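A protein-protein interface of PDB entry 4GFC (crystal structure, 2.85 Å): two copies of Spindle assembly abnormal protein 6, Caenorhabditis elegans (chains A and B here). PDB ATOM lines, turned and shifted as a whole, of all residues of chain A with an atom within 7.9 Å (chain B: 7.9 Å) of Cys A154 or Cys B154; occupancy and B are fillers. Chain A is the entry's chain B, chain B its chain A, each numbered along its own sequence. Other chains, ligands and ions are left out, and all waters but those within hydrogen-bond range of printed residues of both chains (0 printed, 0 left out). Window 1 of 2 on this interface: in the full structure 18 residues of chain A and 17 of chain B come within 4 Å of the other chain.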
ATOM      1  N   PHE A  63     -11.922  25.900  11.162  1.00  0.00           N
ATOM      2  CA  PHE A  63     -10.764  25.783  12.044  1.00  0.00           C
ATOM      3  C   PHE A  63      -9.742  24.764  11.567  1.00  0.00           C
ATOM      4  O   PHE A  63      -8.545  25.027  11.665  1.00  0.00           O
ATOM      5  CB  PHE A  63     -11.207  25.435  13.472  1.00  0.00           C
ATOM      6  CG  PHE A  63     -12.319  26.303  14.017  1.00  0.00           C
ATOM      7  CD1 PHE A  63     -12.110  27.655  14.269  1.00  0.00           C
ATOM      8  CD2 PHE A  63     -13.574  25.768  14.279  1.00  0.00           C
ATOM      9  CE1 PHE A  63     -13.137  28.455  14.767  1.00  0.00           C
ATOM     10  CE2 PHE A  63     -14.604  26.572  14.780  1.00  0.00           C
ATOM     11  CZ  PHE A  63     -14.373  27.907  15.031  1.00  0.00           C
ATOM     12  N   GLU A  64     -10.199  23.615  11.057  1.00  0.00           N
ATOM     13  CA  GLU A  64      -9.314  22.538  10.589  1.00  0.00           C
ATOM     14  C   GLU A  64      -8.604  22.851   9.237  1.00  0.00           C
ATOM     15  O   GLU A  64      -7.549  22.272   8.974  1.00  0.00           O
ATOM     16  CB  GLU A  64     -10.101  21.230  10.478  1.00  0.00           C
ATOM     17  CG  GLU A  64      -9.282  20.014  10.823  1.00  0.00           C
ATOM     18  CD  GLU A  64     -10.079  18.796  11.243  1.00  0.00           C
ATOM     19  OE1 GLU A  64     -11.323  18.895  11.362  1.00  0.00           O
ATOM     20  OE2 GLU A  64      -9.447  17.743  11.488  1.00  0.00           O
ATOM     21  N   ILE A 147      -1.935  22.160  15.858  1.00  0.00           N
ATOM     22  CA  ILE A 147      -2.174  22.349  17.294  1.00  0.00           C
ATOM     23  C   ILE A 147      -1.907  23.838  17.633  1.00  0.00           C
ATOM     24  O   ILE A 147      -2.777  24.470  18.232  1.00  0.00           O
ATOM     25  CB  ILE A 147      -1.355  21.333  18.153  1.00  0.00           C
ATOM     26  CG1 ILE A 147      -1.857  19.885  17.900  1.00  0.00           C
ATOM     27  CG2 ILE A 147      -1.461  21.659  19.626  1.00  0.00           C
ATOM     28  CD1 ILE A 147      -0.892  18.740  18.202  1.00  0.00           C
ATOM     29  N   SER A 148      -0.773  24.417  17.162  1.00  0.00           N
ATOM     30  CA  SER A 148      -0.437  25.840  17.375  1.00  0.00           C
ATOM     31  C   SER A 148      -1.548  26.755  16.853  1.00  0.00           C
ATOM     32  O   SER A 148      -1.951  27.677  17.562  1.00  0.00           O
ATOM     33  CB  SER A 148       0.879  26.200  16.695  1.00  0.00           C
ATOM     34  OG  SER A 148       1.919  25.315  17.082  1.00  0.00           O
ATOM     35  N   HIS A 149      -2.068  26.463  15.641  1.00  0.00           N
ATOM     36  CA  HIS A 149      -3.158  27.181  14.973  1.00  0.00           C
ATOM     37  C   HIS A 149      -4.433  27.160  15.813  1.00  0.00           C
ATOM     38  O   HIS A 149      -4.978  28.221  16.111  1.00  0.00           O
ATOM     39  CB  HIS A 149      -3.421  26.544  13.602  1.00  0.00           C
ATOM     40  CG  HIS A 149      -4.644  27.038  12.881  1.00  0.00           C
ATOM     41  ND1 HIS A 149      -4.633  28.228  12.178  1.00  0.00           N
ATOM     42  CD2 HIS A 149      -5.853  26.447  12.723  1.00  0.00           C
ATOM     43  CE1 HIS A 149      -5.836  28.332  11.640  1.00  0.00           C
ATOM     44  NE2 HIS A 149      -6.598  27.275  11.923  1.00  0.00           N
ATOM     45  N   LEU A 150      -4.897  25.962  16.198  1.00  0.00           N
ATOM     46  CA  LEU A 150      -6.114  25.788  16.972  1.00  0.00           C
ATOM     47  C   LEU A 150      -6.014  26.444  18.331  1.00  0.00           C
ATOM     48  O   LEU A 150      -7.000  27.027  18.785  1.00  0.00           O
ATOM     49  CB  LEU A 150      -6.428  24.304  17.112  1.00  0.00           C
ATOM     50  CG  LEU A 150      -6.925  23.642  15.862  1.00  0.00           C
ATOM     51  CD1 LEU A 150      -6.936  22.163  16.034  1.00  0.00           C
ATOM     52  CD2 LEU A 150      -8.288  24.174  15.470  1.00  0.00           C
ATOM     53  N   LEU A 151      -4.828  26.384  18.971  1.00  0.00           N
ATOM     54  CA  LEU A 151      -4.625  27.017  20.284  1.00  0.00           C
ATOM     55  C   LEU A 151      -4.735  28.533  20.171  1.00  0.00           C
ATOM     56  O   LEU A 151      -5.364  29.152  21.022  1.00  0.00           O
ATOM     57  CB  LEU A 151      -3.279  26.629  20.898  1.00  0.00           C
ATOM     58  CG  LEU A 151      -3.179  25.250  21.513  1.00  0.00           C
ATOM     59  CD1 LEU A 151      -1.760  24.779  21.488  1.00  0.00           C
ATOM     60  CD2 LEU A 151      -3.677  25.259  22.947  1.00  0.00           C
ATOM     61  N   LYS A 152      -4.159  29.120  19.099  1.00  0.00           N
ATOM     62  CA  LYS A 152      -4.230  30.555  18.820  1.00  0.00           C
ATOM     63  C   LYS A 152      -5.693  31.001  18.676  1.00  0.00           C
ATOM     64  O   LYS A 152      -6.036  32.074  19.172  1.00  0.00           O
ATOM     65  CB  LYS A 152      -3.434  30.920  17.557  1.00  0.00           C
ATOM     66  CG  LYS A 152      -1.934  31.044  17.778  1.00  0.00           C
ATOM     67  CD  LYS A 152      -1.224  31.456  16.487  1.00  0.00           C
ATOM     68  CE  LYS A 152       0.207  31.886  16.707  1.00  0.00           C
ATOM     69  NZ  LYS A 152       0.310  33.254  17.288  1.00  0.00           N
ATOM     70  N   ILE A 153      -6.559  30.141  18.064  1.00  0.00           N
ATOM     71  CA  ILE A 153      -8.004  30.374  17.903  1.00  0.00           C
ATOM     72  C   ILE A 153      -8.664  30.330  19.293  1.00  0.00           C
ATOM     73  O   ILE A 153      -9.378  31.259  19.671  1.00  0.00           O
ATOM     74  CB  ILE A 153      -8.672  29.367  16.915  1.00  0.00           C
ATOM     75  CG1 ILE A 153      -8.044  29.444  15.500  1.00  0.00           C
ATOM     76  CG2 ILE A 153     -10.195  29.574  16.850  1.00  0.00           C
ATOM     77  CD1 ILE A 153      -8.413  28.300  14.581  1.00  0.00           C
ATOM     78  N   CYS A 154      -8.397  29.264  20.057  1.00  0.00           N
ATOM     79  CA  CYS A 154      -8.936  29.089  21.398  1.00  0.00           C
ATOM     80  C   CYS A 154      -8.614  30.292  22.272  1.00  0.00           C
ATOM     81  O   CYS A 154      -9.518  30.809  22.920  1.00  0.00           O
ATOM     82  CB  CYS A 154      -8.409  27.799  22.021  1.00  0.00           C
ATOM     83  SG  CYS A 154      -9.201  26.306  21.386  1.00  0.00           S
ATOM     84  N   SER A 155      -7.341  30.743  22.268  1.00  0.00           N
ATOM     85  CA  SER A 155      -6.859  31.882  23.050  1.00  0.00           C
ATOM     86  C   SER A 155      -7.399  33.235  22.515  1.00  0.00           C
ATOM     87  O   SER A 155      -7.524  34.177  23.302  1.00  0.00           O
ATOM     88  CB  SER A 155      -5.334  31.895  23.101  1.00  0.00           C
ATOM     89  OG  SER A 155      -4.756  32.089  21.820  1.00  0.00           O
ATOM     90  N   SER A 156      -7.721  33.336  21.204  1.00  0.00           N
ATOM     91  CA  SER A 156      -8.307  34.564  20.659  1.00  0.00           C
ATOM     92  C   SER A 156      -9.785  34.586  21.035  1.00  0.00           C
ATOM     93  O   SER A 156     -10.256  35.606  21.527  1.00  0.00           O
ATOM     94  CB  SER A 156      -8.091  34.691  19.149  1.00  0.00           C
ATOM     95  OG  SER A 156      -9.022  33.973  18.354  1.00  0.00           O
ATOM     96  N   GLN A 157     -10.486  33.434  20.906  1.00  0.00           N
ATOM     97  CA  GLN A 157     -11.894  33.274  21.293  1.00  0.00           C
ATOM     98  C   GLN A 157     -12.081  33.382  22.820  1.00  0.00           C
ATOM     99  O   GLN A 157     -13.219  33.469  23.290  1.00  0.00           O
ATOM    100  CB  GLN A 157     -12.440  31.920  20.819  1.00  0.00           C
ATOM    101  CG  GLN A 157     -12.709  31.791  19.329  1.00  0.00           C
ATOM    102  CD  GLN A 157     -13.274  30.422  19.000  1.00  0.00           C
ATOM    103  OE1 GLN A 157     -12.739  29.365  19.402  1.00  0.00           O
ATOM    104  NE2 GLN A 157     -14.383  30.411  18.263  1.00  0.00           N
ATOM    105  N   ALA A 158     -10.971  33.315  23.589  1.00  0.00           N
ATOM    106  CA  ALA A 158     -10.957  33.397  25.054  1.00  0.00           C
ATOM    107  C   ALA A 158     -11.056  34.853  25.508  1.00  0.00           C
ATOM    108  O   ALA A 158     -11.792  35.148  26.459  1.00  0.00           O
ATOM    109  CB  ALA A 158      -9.693  32.746  25.607  1.00  0.00           C
ATOM    110  N   VAL A 159     -10.342  35.765  24.793  1.00  0.00           N
ATOM    111  CA  VAL A 159     -10.332  37.217  25.032  1.00  0.00           C
ATOM    112  C   VAL A 159     -11.752  37.765  24.713  1.00  0.00           C
ATOM    113  O   VAL A 159     -12.122  38.852  25.166  1.00  0.00           O
ATOM    114  CB  VAL A 159      -9.196  37.935  24.236  1.00  0.00           C
ATOM    115  CG1 VAL A 159      -9.104  39.414  24.600  1.00  0.00           C
ATOM    116  CG2 VAL A 159      -7.845  37.267  24.476  1.00  0.00           C
ATOM    117  N   LYS A 160     -12.556  36.959  23.983  1.00  0.00           N
ATOM    118  CA  LYS A 160     -13.954  37.216  23.635  1.00  0.00           C
ATOM    119  C   LYS A 160     -14.819  37.141  24.916  1.00  0.00           C
ATOM    120  O   LYS A 160     -15.779  37.896  25.031  1.00  0.00           O
ATOM    121  CB  LYS A 160     -14.407  36.206  22.564  1.00  0.00           C
ATOM    122  CG  LYS A 160     -15.790  36.408  21.967  1.00  0.00           C
ATOM    123  CD  LYS A 160     -16.015  35.389  20.858  1.00  0.00           C
ATOM    124  CE  LYS A 160     -17.433  34.887  20.812  1.00  0.00           C
ATOM    125  NZ  LYS A 160     -17.527  33.571  20.128  1.00  0.00           N
ATOM    126  N   PHE B  63      -6.713  24.962  27.894  1.00  0.00           N
ATOM    127  CA  PHE B  63      -7.051  24.220  26.684  1.00  0.00           C
ATOM    128  C   PHE B  63      -6.029  23.156  26.330  1.00  0.00           C
ATOM    129  O   PHE B  63      -6.428  22.087  25.893  1.00  0.00           O
ATOM    130  CB  PHE B  63      -7.229  25.165  25.485  1.00  0.00           C
ATOM    131  CG  PHE B  63      -8.045  26.411  25.754  1.00  0.00           C
ATOM    132  CD1 PHE B  63      -9.411  26.327  26.024  1.00  0.00           C
ATOM    133  CD2 PHE B  63      -7.448  27.671  25.732  1.00  0.00           C
ATOM    134  CE1 PHE B  63     -10.163  27.481  26.281  1.00  0.00           C
ATOM    135  CE2 PHE B  63      -8.201  28.823  25.977  1.00  0.00           C
ATOM    136  CZ  PHE B  63      -9.551  28.720  26.260  1.00  0.00           C
ATOM    137  N   GLU B  64      -4.733  23.433  26.487  1.00  0.00           N
ATOM    138  CA  GLU B  64      -3.678  22.482  26.117  1.00  0.00           C
ATOM    139  C   GLU B  64      -3.544  21.357  27.140  1.00  0.00           C
ATOM    140  O   GLU B  64      -2.970  20.309  26.802  1.00  0.00           O
ATOM    141  CB  GLU B  64      -2.331  23.196  25.948  1.00  0.00           C
ATOM    142  CG  GLU B  64      -1.447  22.557  24.877  1.00  0.00           C
ATOM    143  CD  GLU B  64      -0.420  23.476  24.250  1.00  0.00           C
ATOM    144  OE1 GLU B  64      -0.405  24.684  24.586  1.00  0.00           O
ATOM    145  OE2 GLU B  64       0.323  23.004  23.361  1.00  0.00           O
ATOM    146  N   ILE B 147      -5.986  17.424  18.856  1.00  0.00           N
ATOM    147  CA  ILE B 147      -6.635  18.172  17.789  1.00  0.00           C
ATOM    148  C   ILE B 147      -8.164  18.066  18.001  1.00  0.00           C
ATOM    149  O   ILE B 147      -8.816  19.107  18.032  1.00  0.00           O
ATOM    150  CB  ILE B 147      -6.152  17.719  16.371  1.00  0.00           C
ATOM    151  CG1 ILE B 147      -4.662  18.062  16.159  1.00  0.00           C
ATOM    152  CG2 ILE B 147      -6.980  18.372  15.277  1.00  0.00           C
ATOM    153  CD1 ILE B 147      -3.935  17.272  15.075  1.00  0.00           C
ATOM    154  N   SER B 148      -8.712  16.850  18.248  1.00  0.00           N
ATOM    155  CA  SER B 148     -10.148  16.655  18.507  1.00  0.00           C
ATOM    156  C   SER B 148     -10.618  17.505  19.682  1.00  0.00           C
ATOM    157  O   SER B 148     -11.641  18.166  19.579  1.00  0.00           O
ATOM    158  CB  SER B 148     -10.460  15.187  18.789  1.00  0.00           C
ATOM    159  OG  SER B 148      -9.955  14.326  17.782  1.00  0.00           O
ATOM    160  N   HIS B 149      -9.834  17.527  20.777  1.00  0.00           N
ATOM    161  CA  HIS B 149     -10.088  18.273  22.007  1.00  0.00           C
ATOM    162  C   HIS B 149     -10.153  19.779  21.734  1.00  0.00           C
ATOM    163  O   HIS B 149     -11.151  20.425  22.071  1.00  0.00           O
ATOM    164  CB  HIS B 149      -8.993  17.946  23.032  1.00  0.00           C
ATOM    165  CG  HIS B 149      -9.046  18.755  24.291  1.00  0.00           C
ATOM    166  ND1 HIS B 149      -9.889  18.413  25.344  1.00  0.00           N
ATOM    167  CD2 HIS B 149      -8.309  19.829  24.651  1.00  0.00           C
ATOM    168  CE1 HIS B 149      -9.649  19.302  26.296  1.00  0.00           C
ATOM    169  NE2 HIS B 149      -8.716  20.180  25.919  1.00  0.00           N
ATOM    170  N   LEU B 150      -9.097  20.319  21.093  1.00  0.00           N
ATOM    171  CA  LEU B 150      -8.944  21.735  20.770  1.00  0.00           C
ATOM    172  C   LEU B 150     -10.011  22.221  19.797  1.00  0.00           C
ATOM    173  O   LEU B 150     -10.448  23.364  19.929  1.00  0.00           O
ATOM    174  CB  LEU B 150      -7.545  22.021  20.226  1.00  0.00           C
ATOM    175  CG  LEU B 150      -6.404  21.913  21.243  1.00  0.00           C
ATOM    176  CD1 LEU B 150      -5.078  22.061  20.587  1.00  0.00           C
ATOM    177  CD2 LEU B 150      -6.541  22.951  22.334  1.00  0.00           C
ATOM    178  N   LEU B 151     -10.470  21.354  18.863  1.00  0.00           N
ATOM    179  CA  LEU B 151     -11.540  21.683  17.914  1.00  0.00           C
ATOM    180  C   LEU B 151     -12.874  21.760  18.627  1.00  0.00           C
ATOM    181  O   LEU B 151     -13.656  22.657  18.317  1.00  0.00           O
ATOM    182  CB  LEU B 151     -11.636  20.664  16.771  1.00  0.00           C
ATOM    183  CG  LEU B 151     -10.599  20.759  15.663  1.00  0.00           C
ATOM    184  CD1 LEU B 151     -10.452  19.425  14.996  1.00  0.00           C
ATOM    185  CD2 LEU B 151     -10.955  21.817  14.639  1.00  0.00           C
ATOM    186  N   LYS B 152     -13.135  20.829  19.586  1.00  0.00           N
ATOM    187  CA  LYS B 152     -14.374  20.792  20.386  1.00  0.00           C
ATOM    188  C   LYS B 152     -14.541  22.097  21.166  1.00  0.00           C
ATOM    189  O   LYS B 152     -15.652  22.612  21.229  1.00  0.00           O
ATOM    190  CB  LYS B 152     -14.408  19.585  21.327  1.00  0.00           C
ATOM    191  CG  LYS B 152     -14.833  18.291  20.645  1.00  0.00           C
ATOM    192  CD  LYS B 152     -14.873  17.135  21.639  1.00  0.00           C
ATOM    193  CE  LYS B 152     -15.622  15.934  21.111  1.00  0.00           C
ATOM    194  NZ  LYS B 152     -17.099  16.089  21.260  1.00  0.00           N
ATOM    195  N   ILE B 153     -13.430  22.652  21.698  1.00  0.00           N
ATOM    196  CA  ILE B 153     -13.377  23.929  22.417  1.00  0.00           C
ATOM    197  C   ILE B 153     -13.720  25.075  21.434  1.00  0.00           C
ATOM    198  O   ILE B 153     -14.607  25.885  21.744  1.00  0.00           O
ATOM    199  CB  ILE B 153     -12.003  24.150  23.121  1.00  0.00           C
ATOM    200  CG1 ILE B 153     -11.724  23.043  24.181  1.00  0.00           C
ATOM    201  CG2 ILE B 153     -11.941  25.552  23.734  1.00  0.00           C
ATOM    202  CD1 ILE B 153     -10.452  23.142  24.953  1.00  0.00           C
ATOM    203  N   CYS B 154     -13.039  25.117  20.246  1.00  0.00           N
ATOM    204  CA  CYS B 154     -13.252  26.108  19.179  1.00  0.00           C
ATOM    205  C   CYS B 154     -14.717  26.129  18.730  1.00  0.00           C
ATOM    206  O   CYS B 154     -15.309  27.202  18.654  1.00  0.00           O
ATOM    207  CB  CYS B 154     -12.322  25.841  17.999  1.00  0.00           C
ATOM    208  SG  CYS B 154     -10.605  26.355  18.268  1.00  0.00           S
ATOM    209  N   SER B 155     -15.296  24.937  18.471  1.00  0.00           N
ATOM    210  CA  SER B 155     -16.689  24.757  18.060  1.00  0.00           C
ATOM    211  C   SER B 155     -17.672  25.054  19.220  1.00  0.00           C
ATOM    212  O   SER B 155     -18.819  25.423  18.952  1.00  0.00           O
ATOM    213  CB  SER B 155     -16.915  23.351  17.513  1.00  0.00           C
ATOM    214  OG  SER B 155     -16.752  22.355  18.508  1.00  0.00           O
ATOM    215  N   SER B 156     -17.226  24.908  20.500  1.00  0.00           N
ATOM    216  CA  SER B 156     -18.070  25.248  21.650  1.00  0.00           C
ATOM    217  C   SER B 156     -18.089  26.764  21.806  1.00  0.00           C
ATOM    218  O   SER B 156     -19.160  27.341  21.988  1.00  0.00           O
ATOM    219  CB  SER B 156     -17.600  24.561  22.931  1.00  0.00           C
ATOM    220  OG  SER B 156     -16.703  25.349  23.700  1.00  0.00           O
ATOM    221  N   GLN B 157     -16.906  27.406  21.683  1.00  0.00           N
ATOM    222  CA  GLN B 157     -16.732  28.866  21.734  1.00  0.00           C
ATOM    223  C   GLN B 157     -17.366  29.561  20.500  1.00  0.00           C
ATOM    224  O   GLN B 157     -17.491  30.789  20.476  1.00  0.00           O
ATOM    225  CB  GLN B 157     -15.243  29.227  21.809  1.00  0.00           C
ATOM    226  CG  GLN B 157     -14.590  28.964  23.151  1.00  0.00           C
ATOM    227  CD  GLN B 157     -13.133  29.354  23.148  1.00  0.00           C
ATOM    228  OE1 GLN B 157     -12.347  28.946  22.283  1.00  0.00           O
ATOM    229  NE2 GLN B 157     -12.733  30.138  24.135  1.00  0.00           N
ATOM    230  N   ALA B 158     -17.723  28.769  19.465  1.00  0.00           N
ATOM    231  CA  ALA B 158     -18.347  29.244  18.230  1.00  0.00           C
ATOM    232  C   ALA B 158     -19.853  29.452  18.439  1.00  0.00           C
ATOM    233  O   ALA B 158     -20.403  30.453  17.967  1.00  0.00           O
ATOM    234  CB  ALA B 158     -18.092  28.258  17.096  1.00  0.00           C
ATOM    235  N   VAL B 159     -20.503  28.524  19.186  1.00  0.00           N
ATOM    236  CA  VAL B 159     -21.931  28.566  19.547  1.00  0.00           C
ATOM    237  C   VAL B 159     -22.157  29.788  20.488  1.00  0.00           C
ATOM    238  O   VAL B 159     -23.285  30.262  20.639  1.00  0.00           O
ATOM    239  CB  VAL B 159     -22.423  27.215  20.158  1.00  0.00           C
ATOM    240  CG1 VAL B 159     -23.930  27.220  20.406  1.00  0.00           C
ATOM    241  CG2 VAL B 159     -22.055  26.036  19.256  1.00  0.00           C
ATOM    242  N   LYS B 160     -21.052  30.325  21.051  1.00  0.00           N
ATOM    243  CA  LYS B 160     -20.998  31.522  21.888  1.00  0.00           C
ATOM    244  C   LYS B 160     -21.320  32.759  21.017  1.00  0.00           C
ATOM    245  O   LYS B 160     -21.954  33.686  21.512  1.00  0.00           O
ATOM    246  CB  LYS B 160     -19.615  31.619  22.554  1.00  0.00           C
ATOM    247  CG  LYS B 160     -19.414  32.728  23.569  1.00  0.00           C
ATOM    248  CD  LYS B 160     -18.031  32.600  24.192  1.00  0.00           C
ATOM    249  CE  LYS B 160     -17.360  33.930  24.430  1.00  0.00           C
ATOM    250  NZ  LYS B 160     -15.889  33.776  24.584  1.00  0.00           N
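The backbone carbonyl oxygen of Leu B150 is in hydrogen-bond range of the side-chain sulfur of Cys A154, 3.5 Å away. The backbone carbonyl oxygen (O) of Leu A150 lies within hydrogen-bond range of the side-chain sulfur (SG) of Cys B154 (3.7 Å). The side-chain sulfur (SG) of Cys B154 lies within hydrogen-bond range of the side-chain sulfur (SG) of Cys A154 (3.4 Å). The backbone carbonyl oxygen of Cys B154 sits at hydrogen-bond distance from the side-chain amide nitrogen of Gln A157 (3.4 Å). The side-chain amide oxygen (OE1) of Gln B157 lies close to the backbone carbonyl oxygen (O) of Cys A154. The side-chain amide oxygen of Gln A157 lies close to the side-chain amide oxygen of Gln B157 (2.9 Å). The backbone carbonyl oxygen (O) of Gln B157 lies within hydrogen-bond range of the side-chain amino group (NZ) of Lys A160 (2.8 Å). The side-chain amino group (NZ) of Lys B160 is in hydrogen-bond range of the backbone carbonyl oxygen (O) of Gln A157, 3.0 Å away.
The backbone carbonyl oxygen of Phe B63 lies within hydrogen-bond range of a ring nitrogen (NE2) of His B149, at 3.0 Å. The backbone carbonyl oxygen (O) of Leu B150 lies within hydrogen-bond range of the side-chain sulfur (SG) of Cys B154. OG of Ser B156 sits at hydrogen-bond distance from O of Ile B153 (2.9 Å). O of Phe A63 is in hydrogen-bond range of NE2 of His A149, at 3.0 Å. The backbone carbonyl oxygen of Leu A150 is in hydrogen-bond range of the side-chain sulfur of Cys A154 (3.5 Å). The backbone carbonyl oxygen (O) of Leu A151 sits at hydrogen-bond distance from the side-chain hydroxyl (OG) of Ser A155 (3.1 Å).
Phe A63 touches Leu B151. Cys B154 touches Phe A63 (O to CZ, 3.8 Å). Ile A147 touches Ile B147 (CG1 to CG1, 3.8 Å). Leu A150 touches Ile B147 (CD1 to CG2, 3.9 Å). Leu A150 touches Leu B151 (CD2 to CD2, 3.7 Å). OE2 of Glu B64 touches CD1 of Leu A151, at 3.3 Å. SG of Cys B154 touches CG2 of Ile A153, 3.5 Å away. Cys A154 touches Ile B153. Ala B158 touches Gln A157. CB of Lys A160 touches NZ of Lys B160 (3.5 Å).
Printed residues of chain B within 4 Å of Phe A63: Leu B151 and Cys B154. Of the printed residues of chain B, Ile A153 touches Cys B154. Of the printed residues of chain A, Leu B151 touches Phe A63 (3.8 Å), Glu A64 (3.8 Å) and Leu A150 (3.7 Å). Printed residues of chain A within 4 Å of Cys B154: Phe A63, Leu A150, Ile A153, Cys A154 and Gln A157. The nearest residue of chain B that does not touch Cys A154 is Leu B151 (5.7 Å). The nearest residue of chain A that does not touch Cys B154 is Leu A151 (5.8 Å). The nearest printed residue of chain A that does not touch Leu B151 is Cys A154 (5.7 Å).
Hydrophobic or aromatic side chains of chain A that line the printed part of chain B: Phe A63, Ile A147, Leu A150, Leu A151 and Ile A153. Of the 16 printed residues of chain B, 10 touch a printed residue of chain A. Along chain B the printed residues that touch a printed residue of chain A span positions 63 to 160. Among the printed residues, 23 pairs touch across the chains. Among the printed residues, no Asp or Glu carboxylate lies within 4 Å of a Lys or Arg side-chain nitrogen of the other chain.
Phe A63 touches Leu B151, but with the chains exchanged Leu A151 does not touch Phe B63 (4.4 Å). Glu A64 touches Leu B151, and with the chains exchanged Leu A151 touches Glu B64. Leu A150 touches Cys B154, and with the chains exchanged Cys A154 touches Leu B150. Gln B157 touches its own counterpart, Gln A157. Positions printed for both chains: 63, 64, 147, 148, 149, 150, 151, 152, 153, 154, 155, 156, 157, 158, 159 and 160.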
